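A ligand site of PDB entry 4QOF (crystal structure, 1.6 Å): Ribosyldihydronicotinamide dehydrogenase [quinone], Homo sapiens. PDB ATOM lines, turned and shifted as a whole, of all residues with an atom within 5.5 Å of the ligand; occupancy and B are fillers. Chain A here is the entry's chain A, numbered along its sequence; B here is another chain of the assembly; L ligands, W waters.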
ATOM      1  N   HIS A  12      23.033  11.363 -23.522  1.00  0.00           N
ATOM      2  CA  HIS A  12      23.137  10.140 -22.732  1.00  0.00           C
ATOM      3  C   HIS A  12      23.352   8.961 -23.645  1.00  0.00           C
ATOM      4  O   HIS A  12      22.722   8.870 -24.714  1.00  0.00           O
ATOM      5  CB  HIS A  12      21.956   9.904 -21.783  1.00  0.00           C
ATOM      6  CG  HIS A  12      22.303   8.992 -20.637  1.00  0.00           C
ATOM      7  ND1 HIS A  12      22.499   7.617 -20.827  1.00  0.00           N
ATOM      8  CD2 HIS A  12      22.536   9.291 -19.333  1.00  0.00           C
ATOM      9  CE1 HIS A  12      22.841   7.138 -19.639  1.00  0.00           C
ATOM     10  NE2 HIS A  12      22.851   8.094 -18.711  1.00  0.00           N
ATOM     11  N   SER A  17      18.184   4.513 -19.829  1.00  0.00           N
ATOM     12  CA  SER A  17      18.547   5.292 -18.636  1.00  0.00           C
ATOM     13  C   SER A  17      17.436   6.208 -18.155  1.00  0.00           C
ATOM     14  O   SER A  17      16.470   6.470 -18.877  1.00  0.00           O
ATOM     15  CB  SER A  17      19.788   6.140 -18.911  1.00  0.00           C
ATOM     16  OG  SER A  17      19.508   7.217 -19.810  1.00  0.00           O
ATOM     17  N   PHE A  18      17.607   6.748 -16.936  1.00  0.00           N
ATOM     18  CA  PHE A  18      16.712   7.725 -16.339  1.00  0.00           C
ATOM     19  C   PHE A  18      16.703   8.998 -17.250  1.00  0.00           C
ATOM     20  O   PHE A  18      15.625   9.531 -17.526  1.00  0.00           O
ATOM     21  CB  PHE A  18      17.172   8.053 -14.917  1.00  0.00           C
ATOM     22  CG  PHE A  18      16.337   9.083 -14.202  1.00  0.00           C
ATOM     23  CD1 PHE A  18      15.089   8.751 -13.685  1.00  0.00           C
ATOM     24  CD2 PHE A  18      16.803  10.376 -14.042  1.00  0.00           C
ATOM     25  CE1 PHE A  18      14.320   9.718 -13.018  1.00  0.00           C
ATOM     26  CE2 PHE A  18      16.040  11.327 -13.357  1.00  0.00           C
ATOM     27  CZ  PHE A  18      14.807  10.999 -12.859  1.00  0.00           C
ATOM     28  N   ASN A  19      17.881   9.405 -17.778  1.00  0.00           N
ATOM     29  CA  ASN A  19      17.968  10.522 -18.731  1.00  0.00           C
ATOM     30  C   ASN A  19      17.117  10.206 -19.971  1.00  0.00           C
ATOM     31  O   ASN A  19      16.351  11.051 -20.416  1.00  0.00           O
ATOM     32  CB  ASN A  19      19.403  10.801 -19.135  1.00  0.00           C
ATOM     33  CG  ASN A  19      20.023  11.846 -18.242  1.00  0.00           C
ATOM     34  OD1 ASN A  19      19.985  13.045 -18.549  1.00  0.00           O
ATOM     35  ND2 ASN A  19      20.558  11.407 -17.113  1.00  0.00           N
ATOM     36  N   GLY A  20      17.216   8.957 -20.458  1.00  0.00           N
ATOM     37  CA  GLY A  20      16.428   8.473 -21.582  1.00  0.00           C
ATOM     38  C   GLY A  20      14.940   8.622 -21.300  1.00  0.00           C
ATOM     39  O   GLY A  20      14.190   9.138 -22.133  1.00  0.00           O
ATOM     40  N   PRO A 103      23.088  14.178 -17.905  1.00  0.00           N
ATOM     41  CA  PRO A 103      23.611  13.904 -16.550  1.00  0.00           C
ATOM     42  C   PRO A 103      24.737  14.914 -16.257  1.00  0.00           C
ATOM     43  O   PRO A 103      25.522  15.256 -17.165  1.00  0.00           O
ATOM     44  CB  PRO A 103      24.194  12.488 -16.675  1.00  0.00           C
ATOM     45  CG  PRO A 103      24.609  12.358 -18.117  1.00  0.00           C
ATOM     46  CD  PRO A 103      23.704  13.292 -18.924  1.00  0.00           C
ATOM     47  N   LEU A 104      24.827  15.377 -15.002  1.00  0.00           N
ATOM     48  CA  LEU A 104      25.872  16.312 -14.598  1.00  0.00           C
ATOM     49  C   LEU A 104      27.211  15.582 -14.588  1.00  0.00           C
ATOM     50  O   LEU A 104      27.350  14.526 -13.930  1.00  0.00           O
ATOM     51  CB  LEU A 104      25.558  16.883 -13.197  1.00  0.00           C
ATOM     52  CG  LEU A 104      26.349  18.125 -12.746  1.00  0.00           C
ATOM     53  CD1 LEU A 104      25.964  19.361 -13.530  1.00  0.00           C
ATOM     54  CD2 LEU A 104      26.138  18.389 -11.258  1.00  0.00           C
ATOM     55  N   TYR A 105      28.178  16.095 -15.372  1.00  0.00           N
ATOM     56  CA  TYR A 105      29.539  15.550 -15.406  1.00  0.00           C
ATOM     57  C   TYR A 105      30.466  16.657 -14.917  1.00  0.00           C
ATOM     58  O   TYR A 105      30.562  17.709 -15.563  1.00  0.00           O
ATOM     59  CB  TYR A 105      29.963  15.161 -16.837  1.00  0.00           C
ATOM     60  CG  TYR A 105      29.595  13.781 -17.355  1.00  0.00           C
ATOM     61  CD1 TYR A 105      28.552  13.052 -16.782  1.00  0.00           C
ATOM     62  CD2 TYR A 105      30.226  13.251 -18.476  1.00  0.00           C
ATOM     63  CE1 TYR A 105      28.183  11.799 -17.298  1.00  0.00           C
ATOM     64  CE2 TYR A 105      29.859  12.017 -18.998  1.00  0.00           C
ATOM     65  CZ  TYR A 105      28.833  11.301 -18.413  1.00  0.00           C
ATOM     66  OH  TYR A 105      28.519  10.081 -18.980  1.00  0.00           O
ATOM     67  N   TRP A 106      31.126  16.437 -13.760  1.00  0.00           N
ATOM     68  CA  TRP A 106      32.065  17.398 -13.197  1.00  0.00           C
ATOM     69  C   TRP A 106      31.455  18.801 -13.086  1.00  0.00           C
ATOM     70  O   TRP A 106      32.036  19.771 -13.605  1.00  0.00           O
ATOM     71  CB  TRP A 106      33.404  17.383 -13.966  1.00  0.00           C
ATOM     72  CG  TRP A 106      34.116  16.066 -13.805  1.00  0.00           C
ATOM     73  CD1 TRP A 106      34.536  15.226 -14.795  1.00  0.00           C
ATOM     74  CD2 TRP A 106      34.517  15.473 -12.564  1.00  0.00           C
ATOM     75  NE1 TRP A 106      35.159  14.121 -14.238  1.00  0.00           N
ATOM     76  CE2 TRP A 106      35.137  14.240 -12.869  1.00  0.00           C
ATOM     77  CE3 TRP A 106      34.364  15.837 -11.213  1.00  0.00           C
ATOM     78  CZ2 TRP A 106      35.608  13.375 -11.878  1.00  0.00           C
ATOM     79  CZ3 TRP A 106      34.816  14.972 -10.228  1.00  0.00           C
ATOM     80  CH2 TRP A 106      35.463  13.772 -10.558  1.00  0.00           C
ATOM     81  N   PHE A 107      30.276  18.898 -12.453  1.00  0.00           N
ATOM     82  CA  PHE A 107      29.530  20.150 -12.221  1.00  0.00           C
ATOM     83  C   PHE A 107      29.209  20.884 -13.530  1.00  0.00           C
ATOM     84  O   PHE A 107      28.991  22.099 -13.522  1.00  0.00           O
ATOM     85  CB  PHE A 107      30.323  21.072 -11.273  1.00  0.00           C
ATOM     86  CG  PHE A 107      30.155  20.862  -9.781  1.00  0.00           C
ATOM     87  CD1 PHE A 107      29.886  19.607  -9.257  1.00  0.00           C
ATOM     88  CD2 PHE A 107      30.291  21.931  -8.898  1.00  0.00           C
ATOM     89  CE1 PHE A 107      29.738  19.414  -7.874  1.00  0.00           C
ATOM     90  CE2 PHE A 107      30.162  21.739  -7.510  1.00  0.00           C
ATOM     91  CZ  PHE A 107      29.879  20.487  -7.013  1.00  0.00           C
ATOM     92  N   SER A 108      29.167  20.154 -14.651  1.00  0.00           N
ATOM     93  CA  SER A 108      28.939  20.756 -15.956  1.00  0.00           C
ATOM     94  C   SER A 108      28.259  19.743 -16.898  1.00  0.00           C
ATOM     95  O   SER A 108      27.740  18.714 -16.452  1.00  0.00           O
ATOM     96  CB  SER A 108      30.281  21.235 -16.517  1.00  0.00           C
ATOM     97  OG  SER A 108      30.242  21.905 -17.760  1.00  0.00           O
ATOM     98  N   THR A 148      20.454  15.774 -14.334  1.00  0.00           N
ATOM     99  CA  THR A 148      20.362  14.685 -13.360  1.00  0.00           C
ATOM    100  C   THR A 148      21.704  14.642 -12.617  1.00  0.00           C
ATOM    101  O   THR A 148      22.738  14.932 -13.222  1.00  0.00           O
ATOM    102  CB  THR A 148      20.010  13.336 -14.014  1.00  0.00           C
ATOM    103  OG1 THR A 148      21.100  12.883 -14.805  1.00  0.00           O
ATOM    104  CG2 THR A 148      18.759  13.413 -14.862  1.00  0.00           C
ATOM    105  N   THR A 149      21.686  14.275 -11.326  1.00  0.00           N
ATOM    106  CA  THR A 149      22.948  14.256 -10.559  1.00  0.00           C
ATOM    107  C   THR A 149      23.222  12.919  -9.859  1.00  0.00           C
ATOM    108  O   THR A 149      22.294  12.138  -9.629  1.00  0.00           O
ATOM    109  CB  THR A 149      22.898  15.345  -9.451  1.00  0.00           C
ATOM    110  OG1 THR A 149      21.883  15.004  -8.498  1.00  0.00           O
ATOM    111  CG2 THR A 149      22.662  16.751  -9.989  1.00  0.00           C
ATOM    112  N   GLY A 150      24.485  12.711  -9.465  1.00  0.00           N
ATOM    113  CA  GLY A 150      24.848  11.594  -8.606  1.00  0.00           C
ATOM    114  C   GLY A 150      24.614  11.997  -7.149  1.00  0.00           C
ATOM    115  O   GLY A 150      24.080  11.214  -6.353  1.00  0.00           O
ATOM    116  N   GLY A 151      24.965  13.243  -6.831  1.00  0.00           N
ATOM    117  CA  GLY A 151      24.804  13.823  -5.499  1.00  0.00           C
ATOM    118  C   GLY A 151      23.359  14.107  -5.109  1.00  0.00           C
ATOM    119  O   GLY A 151      22.517  14.365  -5.981  1.00  0.00           O
ATOM    120  N   TYR A 156      23.783  19.369  -2.425  1.00  0.00           N
ATOM    121  CA  TYR A 156      23.669  20.561  -3.251  1.00  0.00           C
ATOM    122  C   TYR A 156      22.957  21.728  -2.569  1.00  0.00           C
ATOM    123  O   TYR A 156      22.112  22.394  -3.173  1.00  0.00           O
ATOM    124  CB  TYR A 156      23.050  20.240  -4.622  1.00  0.00           C
ATOM    125  CG  TYR A 156      24.038  19.549  -5.526  1.00  0.00           C
ATOM    126  CD1 TYR A 156      25.087  20.250  -6.121  1.00  0.00           C
ATOM    127  CD2 TYR A 156      23.958  18.179  -5.772  1.00  0.00           C
ATOM    128  CE1 TYR A 156      26.013  19.619  -6.953  1.00  0.00           C
ATOM    129  CE2 TYR A 156      24.871  17.531  -6.592  1.00  0.00           C
ATOM    130  CZ  TYR A 156      25.892  18.251  -7.200  1.00  0.00           C
ATOM    131  OH  TYR A 156      26.815  17.644  -8.020  1.00  0.00           O
ATOM    132  N   ASN A 162      28.865  20.050  -1.730  1.00  0.00           N
ATOM    133  CA  ASN A 162      28.902  20.498  -3.129  1.00  0.00           C
ATOM    134  C   ASN A 162      28.511  21.958  -3.325  1.00  0.00           C
ATOM    135  O   ASN A 162      28.664  22.476  -4.433  1.00  0.00           O
ATOM    136  CB  ASN A 162      28.002  19.611  -3.988  1.00  0.00           C
ATOM    137  CG  ASN A 162      28.474  18.189  -4.163  1.00  0.00           C
ATOM    138  OD1 ASN A 162      29.658  17.860  -4.012  1.00  0.00           O
ATOM    139  ND2 ASN A 162      27.554  17.317  -4.532  1.00  0.00           N
ATOM    140  N   PRO A 193      18.986   9.972  -9.076  1.00  0.00           N
ATOM    141  CA  PRO A 193      18.043   8.896  -9.471  1.00  0.00           C
ATOM    142  C   PRO A 193      18.544   7.465  -9.221  1.00  0.00           C
ATOM    143  O   PRO A 193      17.717   6.586  -8.942  1.00  0.00           O
ATOM    144  CB  PRO A 193      17.848   9.143 -10.966  1.00  0.00           C
ATOM    145  CG  PRO A 193      19.081   9.901 -11.398  1.00  0.00           C
ATOM    146  CD  PRO A 193      19.331  10.813 -10.248  1.00  0.00           C
ATOM    147  N   GLU A 194      19.877   7.217  -9.350  1.00  0.00           N
ATOM    148  CA  GLU A 194      20.465   5.889  -9.154  1.00  0.00           C
ATOM    149  C   GLU A 194      20.272   5.382  -7.713  1.00  0.00           C
ATOM    150  O   GLU A 194      20.092   4.176  -7.518  1.00  0.00           O
ATOM    151  CB  GLU A 194      21.963   5.883  -9.480  1.00  0.00           C
ATOM    152  CG  GLU A 194      22.297   6.281 -10.900  1.00  0.00           C
ATOM    153  CD  GLU A 194      23.796   6.434 -11.082  1.00  0.00           C
ATOM    154  OE1 GLU A 194      24.317   7.546 -10.815  1.00  0.00           O
ATOM    155  OE2 GLU A 194      24.459   5.407 -11.357  1.00  0.00           O
ATOM    156  N   ASN B  67      25.888   1.875 -18.180  1.00  0.00           N
ATOM    157  CA  ASN B  67      26.071   2.918 -17.167  1.00  0.00           C
ATOM    158  C   ASN B  67      27.564   3.281 -17.213  1.00  0.00           C
ATOM    159  O   ASN B  67      28.409   2.506 -16.758  1.00  0.00           O
ATOM    160  CB  ASN B  67      25.643   2.393 -15.774  1.00  0.00           C
ATOM    161  CG  ASN B  67      25.716   3.411 -14.663  1.00  0.00           C
ATOM    162  OD1 ASN B  67      26.725   4.108 -14.462  1.00  0.00           O
ATOM    163  ND2 ASN B  67      24.668   3.466 -13.860  1.00  0.00           N
ATOM    164  N   TYR B  68      27.886   4.446 -17.812  1.00  0.00           N
ATOM    165  CA  TYR B  68      29.286   4.864 -17.978  1.00  0.00           C
ATOM    166  C   TYR B  68      30.098   4.849 -16.661  1.00  0.00           C
ATOM    167  O   TYR B  68      31.220   4.323 -16.658  1.00  0.00           O
ATOM    168  CB  TYR B  68      29.410   6.218 -18.694  1.00  0.00           C
ATOM    169  CG  TYR B  68      30.840   6.535 -19.079  1.00  0.00           C
ATOM    170  CD1 TYR B  68      31.415   5.992 -20.222  1.00  0.00           C
ATOM    171  CD2 TYR B  68      31.639   7.352 -18.268  1.00  0.00           C
ATOM    172  CE1 TYR B  68      32.742   6.243 -20.571  1.00  0.00           C
ATOM    173  CE2 TYR B  68      32.975   7.626 -18.611  1.00  0.00           C
ATOM    174  CZ  TYR B  68      33.511   7.073 -19.762  1.00  0.00           C
ATOM    175  OH  TYR B  68      34.832   7.290 -20.090  1.00  0.00           O
ATOM    176  N   GLY B  69      29.545   5.428 -15.600  1.00  0.00           N
ATOM    177  CA  GLY B  69      30.206   5.495 -14.298  1.00  0.00           C
ATOM    178  C   GLY B  69      30.535   4.125 -13.724  1.00  0.00           C
ATOM    179  O   GLY B  69      31.683   3.863 -13.366  1.00  0.00           O
ATOM    180  N   ASP B 118      36.357  14.114 -18.019  1.00  0.00           N
ATOM    181  CA  ASP B 118      35.308  13.093 -17.950  1.00  0.00           C
ATOM    182  C   ASP B 118      35.834  11.679 -17.982  1.00  0.00           C
ATOM    183  O   ASP B 118      35.378  10.842 -17.202  1.00  0.00           O
ATOM    184  CB  ASP B 118      34.302  13.271 -19.091  1.00  0.00           C
ATOM    185  CG  ASP B 118      33.546  14.579 -19.087  1.00  0.00           C
ATOM    186  OD1 ASP B 118      33.577  15.297 -18.042  1.00  0.00           O
ATOM    187  OD2 ASP B 118      32.867  14.876 -20.101  1.00  0.00           O
ATOM    188  N   ARG B 119      36.798  11.431 -18.887  1.00  0.00           N
ATOM    189  CA  ARG B 119      37.293  10.086 -19.146  1.00  0.00           C
ATOM    190  C   ARG B 119      38.492   9.638 -18.288  1.00  0.00           C
ATOM    191  O   ARG B 119      38.611   8.456 -17.975  1.00  0.00           O
ATOM    192  CB  ARG B 119      37.630   9.934 -20.646  1.00  0.00           C
ATOM    193  CG  ARG B 119      36.417  10.145 -21.561  1.00  0.00           C
ATOM    194  CD  ARG B 119      36.812  10.161 -23.046  1.00  0.00           C
ATOM    195  NE  ARG B 119      37.194   8.826 -23.503  1.00  0.00           N
ATOM    196  CZ  ARG B 119      38.416   8.481 -23.945  1.00  0.00           C
ATOM    197  NH1 ARG B 119      39.370   9.393 -24.081  1.00  0.00           N
ATOM    198  NH2 ARG B 119      38.664   7.222 -24.290  1.00  0.00           N
ATOM    199  N   GLY B 175      34.445  21.538  -8.007  1.00  0.00           N
ATOM    200  CA  GLY B 175      33.688  20.395  -8.470  1.00  0.00           C
ATOM    201  C   GLY B 175      34.521  19.288  -9.063  1.00  0.00           C
ATOM    202  O   GLY B 175      34.138  18.110  -8.998  1.00  0.00           O
HETATM  203  N1  LIG L   1      27.241  13.653 -10.246  1.00  0.00           N
HETATM  204  C1  LIG L   1      27.265  14.827  -9.527  1.00  0.00           C
HETATM  205  O1  LIG L   1      26.419  15.051  -8.636  1.00  0.00           O
HETATM  206  N2  LIG L   1      28.249  15.777  -9.775  1.00  0.00           N
HETATM  207  C2  LIG L   1      29.289  15.644 -10.696  1.00  0.00           C
HETATM  208  O2  LIG L   1      30.078  16.577 -10.873  1.00  0.00           O
HETATM  209  C3  LIG L   1      29.295  14.375 -11.409  1.00  0.00           C
HETATM  210  N3  LIG L   1      30.285  14.142 -12.257  1.00  0.00           N
HETATM  211  C4  LIG L   1      30.253  12.955 -12.985  1.00  0.00           C
HETATM  212  C5  LIG L   1      31.258  12.715 -13.924  1.00  0.00           C
HETATM  213  C6  LIG L   1      31.254  11.558 -14.720  1.00  0.00           C
HETATM  214  C7  LIG L   1      32.352  11.360 -15.735  1.00  0.00           C
HETATM  215  C8  LIG L   1      30.213  10.615 -14.566  1.00  0.00           C
HETATM  216  C9  LIG L   1      30.146   9.379 -15.429  1.00  0.00           C
HETATM  217  C10 LIG L   1      29.225  10.850 -13.609  1.00  0.00           C
HETATM  218  C11 LIG L   1      29.231  12.004 -12.823  1.00  0.00           C
HETATM  219  N4  LIG L   1      28.202  12.282 -11.870  1.00  0.00           N
HETATM  220  C12 LIG L   1      28.213  13.450 -11.141  1.00  0.00           C
HETATM  221  C13 LIG L   1      27.109  11.314 -11.678  1.00  0.00           C
HETATM  222  C14 LIG L   1      26.046  11.471 -12.762  1.00  0.00           C
HETATM  223  O3  LIG L   1      25.587  12.831 -12.824  1.00  0.00           O
HETATM  224  C15 LIG L   1      24.897  10.492 -12.517  1.00  0.00           C
HETATM  225  O4  LIG L   1      25.429   9.173 -12.611  1.00  0.00           O
HETATM  226  C16 LIG L   1      23.717  10.634 -13.476  1.00  0.00           C
HETATM  227  O5  LIG L   1      23.195  11.963 -13.382  1.00  0.00           O
HETATM  228  C17 LIG L   1      22.617   9.633 -13.221  1.00  0.00           C
HETATM  229  O6  LIG L   1      21.697   9.730 -14.333  1.00  0.00           O
HETATM  230  P1  LIG L   1      21.571   8.450 -15.284  1.00  0.00           P
HETATM  231  O7  LIG L   1      22.929   8.190 -15.924  1.00  0.00           O
HETATM  232  O8  LIG L   1      20.439   8.644 -16.269  1.00  0.00           O
HETATM  233  O9  LIG L   1      21.179   7.248 -14.312  1.00  0.00           O
HETATM  234  O   HOH W   1      25.477   9.141 -16.320  1.00  0.00           O
HETATM  235  O   HOH W   2      19.490   5.350 -15.142  1.00  0.00           O
HETATM  236  O   HOH W   3      31.782  16.200  -8.637  1.00  0.00           O
HETATM  237  O   HOH W   4      30.336   8.538 -11.433  1.00  0.00           O
HETATM  238  O   HOH W   5      28.030   7.723 -12.648  1.00  0.00           O
HETATM  239  O   HOH W   6      24.141   5.781 -16.050  1.00  0.00           O
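The side-chain carboxylate (OE2) of Glu 194 lies within hydrogen-bond range of the side-chain amide nitrogen (ND2) of Asn 67 of chain B, 3.2 Å away.
The backbone carbonyl oxygen (O) of Thr 148 lies within hydrogen-bond range of the backbone NH (N) of Leu 104, at 2.8 Å.
The side-chain hydroxyl of Thr 148 is in hydrogen-bond range of the side-chain amide nitrogen of Asn 19, 2.8 Å away.
A ring nitrogen (ND1) of His 12 is in hydrogen-bond range of the side-chain hydroxyl of Ser 17 (3.2 Å).
The side-chain hydroxyl (OG) of Ser 17 sits close to the backbone NH (N) of Asn 19, 3.4 Å away.
The backbone carbonyl oxygen (O) of Gly 151 sits at hydrogen-bond distance from the side-chain hydroxyl (OG1) of Thr 149 (2.7 Å).
OG of Ser 17 is in hydrogen-bond range of N of Gly 20 (2.9 Å).
The side-chain carboxylate (OE1) of Glu 194 lies within hydrogen-bond range of an oxygen (O4) of the ligand (2.7 Å).
The backbone NH of Leu 104 sits at hydrogen-bond distance from an oxygen (O3) of the ligand, at 3.4 Å.
The backbone carbonyl oxygen (O) of Leu 104 lies within hydrogen-bond range of an oxygen (O3) of the ligand (2.7 Å).
The side-chain hydroxyl (OH) of Tyr 156 is in hydrogen-bond range of an oxygen (O1) of the ligand (2.7 Å).
The backbone carbonyl oxygen (O) of Thr 148 sits at hydrogen-bond distance from an oxygen (O5) of the ligand.
The side-chain hydroxyl (OG1) of Thr 148 sits at hydrogen-bond distance from an oxygen (O5) of the ligand (2.7 Å).
NE2 of His 12 sits at hydrogen-bond distance from O7 of the ligand.
N of Phe 107 lies within hydrogen-bond range of O2 of the ligand (2.8 Å).
The backbone NH (N) of Trp 106 is in hydrogen-bond range of a nitrogen (N3) of the ligand (2.9 Å).
N of Asn 19 is in hydrogen-bond range of O8 of the ligand (3.1 Å).
The side-chain amide nitrogen of Asn 19 is in hydrogen-bond range of an oxygen (O8) of the ligand, at 2.9 Å.
The backbone NH (N) of Gly 151 sits at hydrogen-bond distance from an oxygen (O1) of the ligand.
The backbone NH of Gly 150 lies within hydrogen-bond range of a nitrogen (N1) of the ligand, 3.0 Å away.
An oxygen (O5) of the ligand is in hydrogen-bond range of the backbone NH (N) of Thr 149.
An oxygen (O8) of the ligand lies within hydrogen-bond range of the backbone NH of Phe 18 (3.5 Å).
Water W2 bridges O9 of the ligand (2.7 Å) and N of Phe 18 (3.0 Å).
Water W6 bridges an oxygen (O7) of the ligand and the side-chain amide nitrogen of Asn 67 of chain B.
Water W3 bridges an oxygen (O2) of the ligand (2.8 Å) and the backbone carbonyl oxygen of Gly 175 of chain B (3.1 Å).
Ser 17 touches the ligand.
CB of Pro 103 touches O5 of the ligand (3.5 Å).
Tyr 105 touches the ligand (CA to N3, 3.5 Å).
Pro 193 touches the ligand.
CD2 of Tyr 68 of chain B touches C9 of the ligand, 3.8 Å away.
Asp 118 of chain B touches the ligand.
Hydrophobic or aromatic side chains within 4 Å of the ligand: His 12, Phe 18, Pro 103, Leu 104, Tyr 105, Phe 107, Tyr 156, Pro 193 and Tyr 68 of chain B.
Along chain A the residues within 4 Å of the ligand span positions 12 to 194.
The nearest printed residue that does not touch the ligand is Gly 69 of chain B (4.0001 Å).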
